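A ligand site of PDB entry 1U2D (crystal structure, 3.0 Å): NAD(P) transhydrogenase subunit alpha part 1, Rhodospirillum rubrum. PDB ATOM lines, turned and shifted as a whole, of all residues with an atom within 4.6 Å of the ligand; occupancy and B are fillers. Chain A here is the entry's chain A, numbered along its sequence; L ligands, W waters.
NH2 of Arg 127 lies within salt-bridge range of O9 of the ligand (3.1 Å). An oxygen (O6) of the ligand sits at hydrogen-bond distance from the guanidinium group (NE) of Arg 204. The side-chain amide oxygen (OE1) of Gln 247 lies close to a nitrogen (N4) of the ligand (3.0 Å). N of Val 182 lies within hydrogen-bond range of O8 of the ligand. The backbone NH (N) of Gly 181 sits close to an oxygen (O5) of the ligand (3.4 Å). An oxygen (O14) of the ligand sits at hydrogen-bond distance from the side-chain amide nitrogen of Gln 132 (3.1 Å). OD1 of Asp 202 sits at hydrogen-bond distance from O6 of the ligand (2.6 Å). N7 of the ligand is in hydrogen-bond range of O of Ile 128, at 3.4 Å.
Merely in contact with the ligand: Ala 265 (3.2 Å), Ala 236 (3.4 Å), Val 203 (3.5 Å), Thr 264 (3.5 Å), Leu 266 (3.5 Å), Ser 138 (3.5 Å), Gly 234 (3.5 Å), Pro 273 (3.6 Å), Val 180 (3.7 Å), Leu 275 (3.7 Å), Asp 135 (3.8 Å), Gly 179 (3.8 Å) and Ile 267 (3.9 Å). Hydrophobic or aromatic side chains that line the ligand: Val 182, Val 203, Ala 236, Ala 265, Leu 266, Ile 267, Pro 273 and Leu 275. The nearest printed residue that does not touch the ligand is Pro 126 (4.04 Å).
The side-chain hydroxyl (OG1) of Thr 264 is in hydrogen-bond range of the backbone carbonyl oxygen (O) of Gly 179. N of Ser 138 is in hydrogen-bond range of OD1 of Asp 135. OD1 of Asp 202 lies close to N of Arg 204 (3.4 Å). N of Val 180 lies within hydrogen-bond range of OD2 of Asp 202. The backbone carbonyl oxygen of Gly 234 lies close to the guanidinium group of Arg 204 (3.4 Å). The backbone carbonyl oxygen (O) of Thr 201 lies within hydrogen-bond range of the backbone NH (N) of Gly 179 (3.0 Å). The side-chain hydroxyl of Ser 141 lies within hydrogen-bond range of the backbone carbonyl oxygen of Ser 138, at 3.1 Å.
Water W1 lies within hydrogen-bond range of O2 of the ligand, N of Ala 236 and O of Leu 266.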
ATOM      1  N   PRO A 126     -14.620 -34.688 -24.152  1.00  0.00           N
ATOM      2  CA  PRO A 126     -15.768 -33.893 -23.720  1.00  0.00           C
ATOM      3  C   PRO A 126     -16.129 -34.114 -22.238  1.00  0.00           C
ATOM      4  O   PRO A 126     -15.764 -35.140 -21.664  1.00  0.00           O
ATOM      5  CB  PRO A 126     -16.907 -34.365 -24.635  1.00  0.00           C
ATOM      6  CG  PRO A 126     -16.456 -35.652 -25.204  1.00  0.00           C
ATOM      7  CD  PRO A 126     -14.972 -35.586 -25.272  1.00  0.00           C
ATOM      8  N   ARG A 127     -16.849 -33.160 -21.656  1.00  0.00           N
ATOM      9  CA  ARG A 127     -17.107 -33.141 -20.208  1.00  0.00           C
ATOM     10  C   ARG A 127     -18.349 -33.949 -19.800  1.00  0.00           C
ATOM     11  O   ARG A 127     -19.002 -33.626 -18.803  1.00  0.00           O
ATOM     12  CB  ARG A 127     -17.237 -31.698 -19.713  1.00  0.00           C
ATOM     13  CG  ARG A 127     -16.127 -30.731 -20.164  1.00  0.00           C
ATOM     14  CD  ARG A 127     -14.807 -30.954 -19.440  1.00  0.00           C
ATOM     15  NE  ARG A 127     -14.083 -29.696 -19.240  1.00  0.00           N
ATOM     16  CZ  ARG A 127     -12.899 -29.576 -18.650  1.00  0.00           C
ATOM     17  NH1 ARG A 127     -12.246 -30.648 -18.204  1.00  0.00           N
ATOM     18  NH2 ARG A 127     -12.352 -28.376 -18.517  1.00  0.00           N
ATOM     19  N   ILE A 128     -18.660 -34.994 -20.561  1.00  0.00           N
ATOM     20  CA  ILE A 128     -19.769 -35.907 -20.229  1.00  0.00           C
ATOM     21  C   ILE A 128     -19.376 -36.867 -19.111  1.00  0.00           C
ATOM     22  O   ILE A 128     -18.231 -37.321 -19.050  1.00  0.00           O
ATOM     23  CB  ILE A 128     -20.257 -36.717 -21.467  1.00  0.00           C
ATOM     24  CG1 ILE A 128     -19.083 -37.164 -22.345  1.00  0.00           C
ATOM     25  CG2 ILE A 128     -21.251 -35.891 -22.283  1.00  0.00           C
ATOM     26  CD1 ILE A 128     -19.406 -38.303 -23.281  1.00  0.00           C
ATOM     27  N   SER A 129     -20.332 -37.197 -18.248  1.00  0.00           N
ATOM     28  CA  SER A 129     -20.080 -38.000 -17.041  1.00  0.00           C
ATOM     29  C   SER A 129     -19.368 -39.329 -17.305  1.00  0.00           C
ATOM     30  O   SER A 129     -18.509 -39.726 -16.520  1.00  0.00           O
ATOM     31  CB  SER A 129     -21.398 -38.285 -16.304  1.00  0.00           C
ATOM     32  OG  SER A 129     -21.809 -37.158 -15.539  1.00  0.00           O
ATOM     33  N   ALA A 131     -17.240 -40.235 -19.569  1.00  0.00           N
ATOM     34  CA  ALA A 131     -15.863 -40.148 -20.075  1.00  0.00           C
ATOM     35  C   ALA A 131     -14.891 -39.582 -19.043  1.00  0.00           C
ATOM     36  O   ALA A 131     -13.780 -39.170 -19.399  1.00  0.00           O
ATOM     37  CB  ALA A 131     -15.829 -39.308 -21.354  1.00  0.00           C
ATOM     38  N   GLN A 132     -15.284 -39.557 -17.770  1.00  0.00           N
ATOM     39  CA  GLN A 132     -14.395 -39.130 -16.685  1.00  0.00           C
ATOM     40  C   GLN A 132     -13.263 -40.129 -16.476  1.00  0.00           C
ATOM     41  O   GLN A 132     -12.138 -39.741 -16.162  1.00  0.00           O
ATOM     42  CB  GLN A 132     -15.179 -38.950 -15.373  1.00  0.00           C
ATOM     43  CG  GLN A 132     -15.986 -37.666 -15.310  1.00  0.00           C
ATOM     44  CD  GLN A 132     -16.847 -37.558 -14.063  1.00  0.00           C
ATOM     45  OE1 GLN A 132     -16.670 -38.314 -13.110  1.00  0.00           O
ATOM     46  NE2 GLN A 132     -17.784 -36.617 -14.069  1.00  0.00           N
ATOM     47  N   ASP A 135     -10.557 -39.316 -18.945  1.00  0.00           N
ATOM     48  CA  ASP A 135     -10.092 -37.930 -18.964  1.00  0.00           C
ATOM     49  C   ASP A 135      -8.689 -37.811 -18.358  1.00  0.00           C
ATOM     50  O   ASP A 135      -8.468 -38.216 -17.213  1.00  0.00           O
ATOM     51  CB  ASP A 135     -11.080 -37.047 -18.181  1.00  0.00           C
ATOM     52  CG  ASP A 135     -11.127 -35.625 -18.713  1.00  0.00           C
ATOM     53  OD1 ASP A 135     -10.133 -34.890 -18.520  1.00  0.00           O
ATOM     54  OD2 ASP A 135     -12.161 -35.236 -19.299  1.00  0.00           O
ATOM     55  N   SER A 138      -8.229 -34.446 -16.080  1.00  0.00           N
ATOM     56  CA  SER A 138      -8.791 -34.610 -14.750  1.00  0.00           C
ATOM     57  C   SER A 138      -7.889 -35.431 -13.823  1.00  0.00           C
ATOM     58  O   SER A 138      -7.588 -34.998 -12.714  1.00  0.00           O
ATOM     59  CB  SER A 138     -10.174 -35.279 -14.856  1.00  0.00           C
ATOM     60  OG  SER A 138     -11.072 -34.732 -13.919  1.00  0.00           O
ATOM     61  N   SER A 141      -4.654 -33.326 -13.160  1.00  0.00           N
ATOM     62  CA  SER A 141      -4.880 -32.097 -12.402  1.00  0.00           C
ATOM     63  C   SER A 141      -5.167 -32.382 -10.925  1.00  0.00           C
ATOM     64  O   SER A 141      -4.916 -31.542 -10.072  1.00  0.00           O
ATOM     65  CB  SER A 141      -6.009 -31.263 -13.002  1.00  0.00           C
ATOM     66  OG  SER A 141      -7.242 -31.971 -13.002  1.00  0.00           O
ATOM     67  N   GLY A 179      -9.650 -20.829  -7.457  1.00  0.00           N
ATOM     68  CA  GLY A 179     -10.091 -21.826  -8.430  1.00  0.00           C
ATOM     69  C   GLY A 179     -10.265 -23.187  -7.795  1.00  0.00           C
ATOM     70  O   GLY A 179      -9.287 -23.881  -7.527  1.00  0.00           O
ATOM     71  N   VAL A 180     -11.512 -23.567  -7.548  1.00  0.00           N
ATOM     72  CA  VAL A 180     -11.847 -24.825  -6.888  1.00  0.00           C
ATOM     73  C   VAL A 180     -12.292 -25.851  -7.939  1.00  0.00           C
ATOM     74  O   VAL A 180     -13.423 -26.333  -7.921  1.00  0.00           O
ATOM     75  CB  VAL A 180     -12.948 -24.618  -5.837  1.00  0.00           C
ATOM     76  CG1 VAL A 180     -13.129 -25.878  -4.988  1.00  0.00           C
ATOM     77  CG2 VAL A 180     -12.613 -23.431  -4.944  1.00  0.00           C
ATOM     78  N   GLY A 181     -11.373 -26.178  -8.844  1.00  0.00           N
ATOM     79  CA  GLY A 181     -11.611 -27.228  -9.835  1.00  0.00           C
ATOM     80  C   GLY A 181     -11.205 -28.583  -9.270  1.00  0.00           C
ATOM     81  O   GLY A 181     -11.295 -28.808  -8.057  1.00  0.00           O
ATOM     82  N   VAL A 182     -10.748 -29.472 -10.140  1.00  0.00           N
ATOM     83  CA  VAL A 182     -10.225 -30.770  -9.715  1.00  0.00           C
ATOM     84  C   VAL A 182      -8.969 -30.567  -8.862  1.00  0.00           C
ATOM     85  O   VAL A 182      -8.820 -31.189  -7.807  1.00  0.00           O
ATOM     86  CB  VAL A 182      -9.889 -31.682 -10.916  1.00  0.00           C
ATOM     87  CG1 VAL A 182      -9.134 -32.932 -10.471  1.00  0.00           C
ATOM     88  CG2 VAL A 182     -11.164 -32.058 -11.664  1.00  0.00           C
ATOM     89  N   THR A 201     -11.937 -19.574  -3.221  1.00  0.00           N
ATOM     90  CA  THR A 201     -12.920 -18.831  -4.011  1.00  0.00           C
ATOM     91  C   THR A 201     -13.038 -19.378  -5.422  1.00  0.00           C
ATOM     92  O   THR A 201     -12.116 -20.005  -5.940  1.00  0.00           O
ATOM     93  CB  THR A 201     -12.545 -17.336  -4.118  1.00  0.00           C
ATOM     94  OG1 THR A 201     -13.589 -16.636  -4.814  1.00  0.00           O
ATOM     95  CG2 THR A 201     -11.218 -17.129  -4.853  1.00  0.00           C
ATOM     96  N   ASP A 202     -14.188 -19.132  -6.036  1.00  0.00           N
ATOM     97  CA  ASP A 202     -14.431 -19.514  -7.432  1.00  0.00           C
ATOM     98  C   ASP A 202     -15.610 -18.716  -7.977  1.00  0.00           C
ATOM     99  O   ASP A 202     -16.413 -18.176  -7.215  1.00  0.00           O
ATOM    100  CB  ASP A 202     -14.708 -21.014  -7.534  1.00  0.00           C
ATOM    101  CG  ASP A 202     -14.409 -21.575  -8.915  1.00  0.00           C
ATOM    102  OD1 ASP A 202     -14.545 -20.828  -9.916  1.00  0.00           O
ATOM    103  OD2 ASP A 202     -14.048 -22.762  -9.019  1.00  0.00           O
ATOM    104  N   VAL A 203     -15.703 -18.653  -9.303  1.00  0.00           N
ATOM    105  CA  VAL A 203     -16.849 -18.028  -9.980  1.00  0.00           C
ATOM    106  C   VAL A 203     -18.092 -18.929  -9.944  1.00  0.00           C
ATOM    107  O   VAL A 203     -19.216 -18.436  -9.890  1.00  0.00           O
ATOM    108  CB  VAL A 203     -16.522 -17.637 -11.440  1.00  0.00           C
ATOM    109  CG1 VAL A 203     -15.380 -16.638 -11.484  1.00  0.00           C
ATOM    110  CG2 VAL A 203     -16.204 -18.871 -12.309  1.00  0.00           C
ATOM    111  N   ARG A 204     -17.882 -20.245  -9.968  1.00  0.00           N
ATOM    112  CA  ARG A 204     -18.981 -21.213 -10.039  1.00  0.00           C
ATOM    113  C   ARG A 204     -19.586 -21.418  -8.647  1.00  0.00           C
ATOM    114  O   ARG A 204     -18.896 -21.845  -7.716  1.00  0.00           O
ATOM    115  CB  ARG A 204     -18.493 -22.543 -10.612  1.00  0.00           C
ATOM    116  CG  ARG A 204     -17.826 -22.400 -11.982  1.00  0.00           C
ATOM    117  CD  ARG A 204     -17.532 -23.742 -12.649  1.00  0.00           C
ATOM    118  NE  ARG A 204     -16.546 -24.550 -11.938  1.00  0.00           N
ATOM    119  CZ  ARG A 204     -16.827 -25.600 -11.162  1.00  0.00           C
ATOM    120  NH1 ARG A 204     -18.084 -26.022 -10.994  1.00  0.00           N
ATOM    121  NH2 ARG A 204     -15.849 -26.261 -10.561  1.00  0.00           N
ATOM    122  N   GLY A 233     -20.382 -27.524 -20.179  1.00  0.00           N
ATOM    123  CA  GLY A 233     -19.412 -28.549 -19.765  1.00  0.00           C
ATOM    124  C   GLY A 233     -18.973 -28.469 -18.312  1.00  0.00           C
ATOM    125  O   GLY A 233     -18.389 -29.423 -17.782  1.00  0.00           O
ATOM    126  N   GLY A 234     -19.247 -27.338 -17.664  1.00  0.00           N
ATOM    127  CA  GLY A 234     -18.890 -27.135 -16.250  1.00  0.00           C
ATOM    128  C   GLY A 234     -17.674 -26.258 -16.029  1.00  0.00           C
ATOM    129  O   GLY A 234     -17.304 -25.998 -14.885  1.00  0.00           O
ATOM    130  N   TYR A 235     -17.053 -25.806 -17.116  1.00  0.00           N
ATOM    131  CA  TYR A 235     -15.875 -24.923 -17.038  1.00  0.00           C
ATOM    132  C   TYR A 235     -16.287 -23.455 -17.009  1.00  0.00           C
ATOM    133  O   TYR A 235     -17.426 -23.104 -17.331  1.00  0.00           O
ATOM    134  CB  TYR A 235     -14.883 -25.197 -18.183  1.00  0.00           C
ATOM    135  CG  TYR A 235     -15.488 -25.299 -19.565  1.00  0.00           C
ATOM    136  CD1 TYR A 235     -15.736 -24.160 -20.335  1.00  0.00           C
ATOM    137  CD2 TYR A 235     -15.801 -26.538 -20.125  1.00  0.00           C
ATOM    138  CE1 TYR A 235     -16.291 -24.255 -21.605  1.00  0.00           C
ATOM    139  CE2 TYR A 235     -16.356 -26.648 -21.391  1.00  0.00           C
ATOM    140  CZ  TYR A 235     -16.594 -25.502 -22.136  1.00  0.00           C
ATOM    141  OH  TYR A 235     -17.136 -25.605 -23.393  1.00  0.00           O
ATOM    142  N   ALA A 236     -15.341 -22.595 -16.625  1.00  0.00           N
ATOM    143  CA  ALA A 236     -15.625 -21.178 -16.430  1.00  0.00           C
ATOM    144  C   ALA A 236     -15.641 -20.402 -17.747  1.00  0.00           C
ATOM    145  O   ALA A 236     -15.140 -20.874 -18.772  1.00  0.00           O
ATOM    146  CB  ALA A 236     -14.599 -20.566 -15.482  1.00  0.00           C
ATOM    147  N   MET A 239     -15.056 -13.183 -17.104  1.00  0.00           N
ATOM    148  CA  MET A 239     -15.832 -12.399 -16.129  1.00  0.00           C
ATOM    149  C   MET A 239     -15.706 -10.873 -16.296  1.00  0.00           C
ATOM    150  O   MET A 239     -16.524 -10.126 -15.771  1.00  0.00           O
ATOM    151  CB  MET A 239     -15.413 -12.784 -14.701  1.00  0.00           C
ATOM    152  CG  MET A 239     -15.603 -14.262 -14.376  1.00  0.00           C
ATOM    153  SD  MET A 239     -17.304 -14.840 -14.512  1.00  0.00           S
ATOM    154  CE  MET A 239     -18.111 -13.925 -13.203  1.00  0.00           C
ATOM    155  N   GLN A 247     -13.596  -9.058  -6.951  1.00  0.00           N
ATOM    156  CA  GLN A 247     -12.927 -10.267  -6.457  1.00  0.00           C
ATOM    157  C   GLN A 247     -11.588  -9.906  -5.812  1.00  0.00           C
ATOM    158  O   GLN A 247     -11.308 -10.324  -4.689  1.00  0.00           O
ATOM    159  CB  GLN A 247     -12.702 -11.236  -7.616  1.00  0.00           C
ATOM    160  CG  GLN A 247     -12.069 -12.568  -7.214  1.00  0.00           C
ATOM    161  CD  GLN A 247     -11.814 -13.478  -8.396  1.00  0.00           C
ATOM    162  OE1 GLN A 247     -12.161 -14.654  -8.369  1.00  0.00           O
ATOM    163  NE2 GLN A 247     -11.199 -12.929  -9.445  1.00  0.00           N
ATOM    164  N   THR A 264      -5.258 -22.037  -9.450  1.00  0.00           N
ATOM    165  CA  THR A 264      -5.522 -23.117 -10.404  1.00  0.00           C
ATOM    166  C   THR A 264      -6.447 -22.720 -11.559  1.00  0.00           C
ATOM    167  O   THR A 264      -6.794 -23.567 -12.384  1.00  0.00           O
ATOM    168  CB  THR A 264      -6.157 -24.346  -9.694  1.00  0.00           C
ATOM    169  OG1 THR A 264      -7.579 -24.167  -9.571  1.00  0.00           O
ATOM    170  CG2 THR A 264      -5.557 -24.543  -8.303  1.00  0.00           C
ATOM    171  N   ALA A 265      -6.844 -21.453 -11.631  1.00  0.00           N
ATOM    172  CA  ALA A 265      -7.925 -21.026 -12.518  1.00  0.00           C
ATOM    173  C   ALA A 265      -7.547 -21.107 -14.001  1.00  0.00           C
ATOM    174  O   ALA A 265      -6.459 -20.702 -14.401  1.00  0.00           O
ATOM    175  CB  ALA A 265      -8.392 -19.623 -12.167  1.00  0.00           C
ATOM    176  N   LEU A 266      -8.486 -21.622 -14.799  1.00  0.00           N
ATOM    177  CA  LEU A 266      -8.306 -21.810 -16.236  1.00  0.00           C
ATOM    178  C   LEU A 266      -9.604 -21.459 -16.975  1.00  0.00           C
ATOM    179  O   LEU A 266     -10.692 -21.746 -16.481  1.00  0.00           O
ATOM    180  CB  LEU A 266      -7.938 -23.270 -16.527  1.00  0.00           C
ATOM    181  CG  LEU A 266      -6.503 -23.631 -16.954  1.00  0.00           C
ATOM    182  CD1 LEU A 266      -5.446 -22.978 -16.087  1.00  0.00           C
ATOM    183  CD2 LEU A 266      -6.338 -25.145 -16.941  1.00  0.00           C
ATOM    184  N   ILE A 267      -9.474 -20.831 -18.146  1.00  0.00           N
ATOM    185  CA  ILE A 267     -10.627 -20.553 -19.015  1.00  0.00           C
ATOM    186  C   ILE A 267     -10.326 -21.097 -20.418  1.00  0.00           C
ATOM    187  O   ILE A 267      -9.533 -20.499 -21.144  1.00  0.00           O
ATOM    188  CB  ILE A 267     -10.928 -19.039 -19.080  1.00  0.00           C
ATOM    189  CG1 ILE A 267     -11.463 -18.537 -17.738  1.00  0.00           C
ATOM    190  CG2 ILE A 267     -11.958 -18.745 -20.183  1.00  0.00           C
ATOM    191  CD1 ILE A 267     -11.480 -17.029 -17.574  1.00  0.00           C
ATOM    192  N   PRO A 268     -10.956 -22.231 -20.799  1.00  0.00           N
ATOM    193  CA  PRO A 268     -10.717 -22.874 -22.098  1.00  0.00           C
ATOM    194  C   PRO A 268     -10.810 -21.910 -23.276  1.00  0.00           C
ATOM    195  O   PRO A 268     -11.812 -21.202 -23.418  1.00  0.00           O
ATOM    196  CB  PRO A 268     -11.837 -23.920 -22.170  1.00  0.00           C
ATOM    197  CG  PRO A 268     -12.107 -24.263 -20.765  1.00  0.00           C
ATOM    198  CD  PRO A 268     -11.929 -22.992 -19.987  1.00  0.00           C
ATOM    199  N   PRO A 273      -6.932 -16.411 -16.179  1.00  0.00           N
ATOM    200  CA  PRO A 273      -7.309 -15.105 -15.640  1.00  0.00           C
ATOM    201  C   PRO A 273      -6.388 -14.634 -14.526  1.00  0.00           C
ATOM    202  O   PRO A 273      -5.942 -15.448 -13.721  1.00  0.00           O
ATOM    203  CB  PRO A 273      -8.717 -15.350 -15.099  1.00  0.00           C
ATOM    204  CG  PRO A 273      -8.744 -16.780 -14.763  1.00  0.00           C
ATOM    205  CD  PRO A 273      -7.885 -17.459 -15.780  1.00  0.00           C
ATOM    206  N   LEU A 275      -5.652 -13.351 -11.123  1.00  0.00           N
ATOM    207  CA  LEU A 275      -6.299 -13.344  -9.813  1.00  0.00           C
ATOM    208  C   LEU A 275      -5.444 -12.625  -8.766  1.00  0.00           C
ATOM    209  O   LEU A 275      -5.978 -12.027  -7.827  1.00  0.00           O
ATOM    210  CB  LEU A 275      -6.571 -14.776  -9.346  1.00  0.00           C
ATOM    211  CG  LEU A 275      -7.172 -15.706 -10.412  1.00  0.00           C
ATOM    212  CD1 LEU A 275      -7.023 -17.161 -10.002  1.00  0.00           C
ATOM    213  CD2 LEU A 275      -8.625 -15.359 -10.676  1.00  0.00           C
HETATM  214  P1  LIG L   1     -10.484 -25.974 -15.020  1.00  0.00           P
HETATM  215  O1  LIG L   1      -9.164 -26.694 -14.966  1.00  0.00           O
HETATM  216  O2  LIG L   1     -11.120 -25.666 -16.363  1.00  0.00           O
HETATM  217  O3  LIG L   1     -10.372 -24.600 -14.188  1.00  0.00           O
HETATM  218  C1  LIG L   1     -10.095 -24.643 -12.796  1.00  0.00           C
HETATM  219  C2  LIG L   1     -11.073 -23.802 -11.973  1.00  0.00           C
HETATM  220  O4  LIG L   1     -10.789 -22.412 -12.138  1.00  0.00           O
HETATM  221  C3  LIG L   1     -12.546 -23.979 -12.316  1.00  0.00           C
HETATM  222  O5  LIG L   1     -13.235 -24.563 -11.233  1.00  0.00           O
HETATM  223  C4  LIG L   1     -13.064 -22.574 -12.566  1.00  0.00           C
HETATM  224  O6  LIG L   1     -14.356 -22.397 -12.013  1.00  0.00           O
HETATM  225  C5  LIG L   1     -12.011 -21.700 -11.905  1.00  0.00           C
HETATM  226  N1  LIG L   1     -11.938 -20.314 -12.424  1.00  0.00           N
HETATM  227  C6  LIG L   1     -11.790 -19.909 -13.714  1.00  0.00           C
HETATM  228  N2  LIG L   1     -11.740 -18.541 -13.834  1.00  0.00           N
HETATM  229  C7  LIG L   1     -11.856 -18.032 -12.589  1.00  0.00           C
HETATM  230  C8  LIG L   1     -11.890 -16.724 -11.890  1.00  0.00           C
HETATM  231  N3  LIG L   1     -11.790 -15.574 -12.591  1.00  0.00           N
HETATM  232  N4  LIG L   1     -12.035 -16.690 -10.543  1.00  0.00           N
HETATM  233  C9  LIG L   1     -12.143 -17.802  -9.777  1.00  0.00           C
HETATM  234  N5  LIG L   1     -12.120 -19.037 -10.294  1.00  0.00           N
HETATM  235  C10 LIG L   1     -11.977 -19.190 -11.716  1.00  0.00           C
HETATM  236  O7  LIG L   1     -11.565 -26.729 -14.100  1.00  0.00           O
HETATM  237  P2  LIG L   1     -11.705 -28.333 -14.032  1.00  0.00           P
HETATM  238  O8  LIG L   1     -10.560 -28.906 -13.242  1.00  0.00           O
HETATM  239  O9  LIG L   1     -11.996 -28.842 -15.434  1.00  0.00           O
HETATM  240  O10 LIG L   1     -13.050 -28.481 -13.163  1.00  0.00           O
HETATM  241  C11 LIG L   1     -14.202 -27.676 -13.418  1.00  0.00           C
HETATM  242  C12 LIG L   1     -15.454 -28.522 -13.258  1.00  0.00           C
HETATM  243  O11 LIG L   1     -15.566 -29.426 -14.353  1.00  0.00           O
HETATM  244  C13 LIG L   1     -15.438 -29.365 -11.985  1.00  0.00           C
HETATM  245  O12 LIG L   1     -16.693 -29.261 -11.332  1.00  0.00           O
HETATM  246  C14 LIG L   1     -15.182 -30.781 -12.463  1.00  0.00           C
HETATM  247  O13 LIG L   1     -15.807 -31.738 -11.628  1.00  0.00           O
HETATM  248  C15 LIG L   1     -15.733 -30.771 -13.886  1.00  0.00           C
HETATM  249  N6  LIG L   1     -15.054 -31.749 -14.754  1.00  0.00           N
HETATM  250  C16 LIG L   1     -15.778 -32.656 -15.311  1.00  0.00           C
HETATM  251  C17 LIG L   1     -15.296 -33.611 -16.140  1.00  0.00           C
HETATM  252  C18 LIG L   1     -16.192 -34.621 -16.735  1.00  0.00           C
HETATM  253  O14 LIG L   1     -17.363 -34.648 -16.391  1.00  0.00           O
HETATM  254  N7  LIG L   1     -15.766 -35.512 -17.638  1.00  0.00           N
HETATM  255  C19 LIG L   1     -13.814 -33.526 -16.364  1.00  0.00           C
HETATM  256  C20 LIG L   1     -13.057 -32.441 -15.690  1.00  0.00           C
HETATM  257  C21 LIG L   1     -13.773 -31.626 -14.910  1.00  0.00           C
HETATM  258  O   HOH W   1     -12.792 -23.644 -16.231  1.00  0.00           O
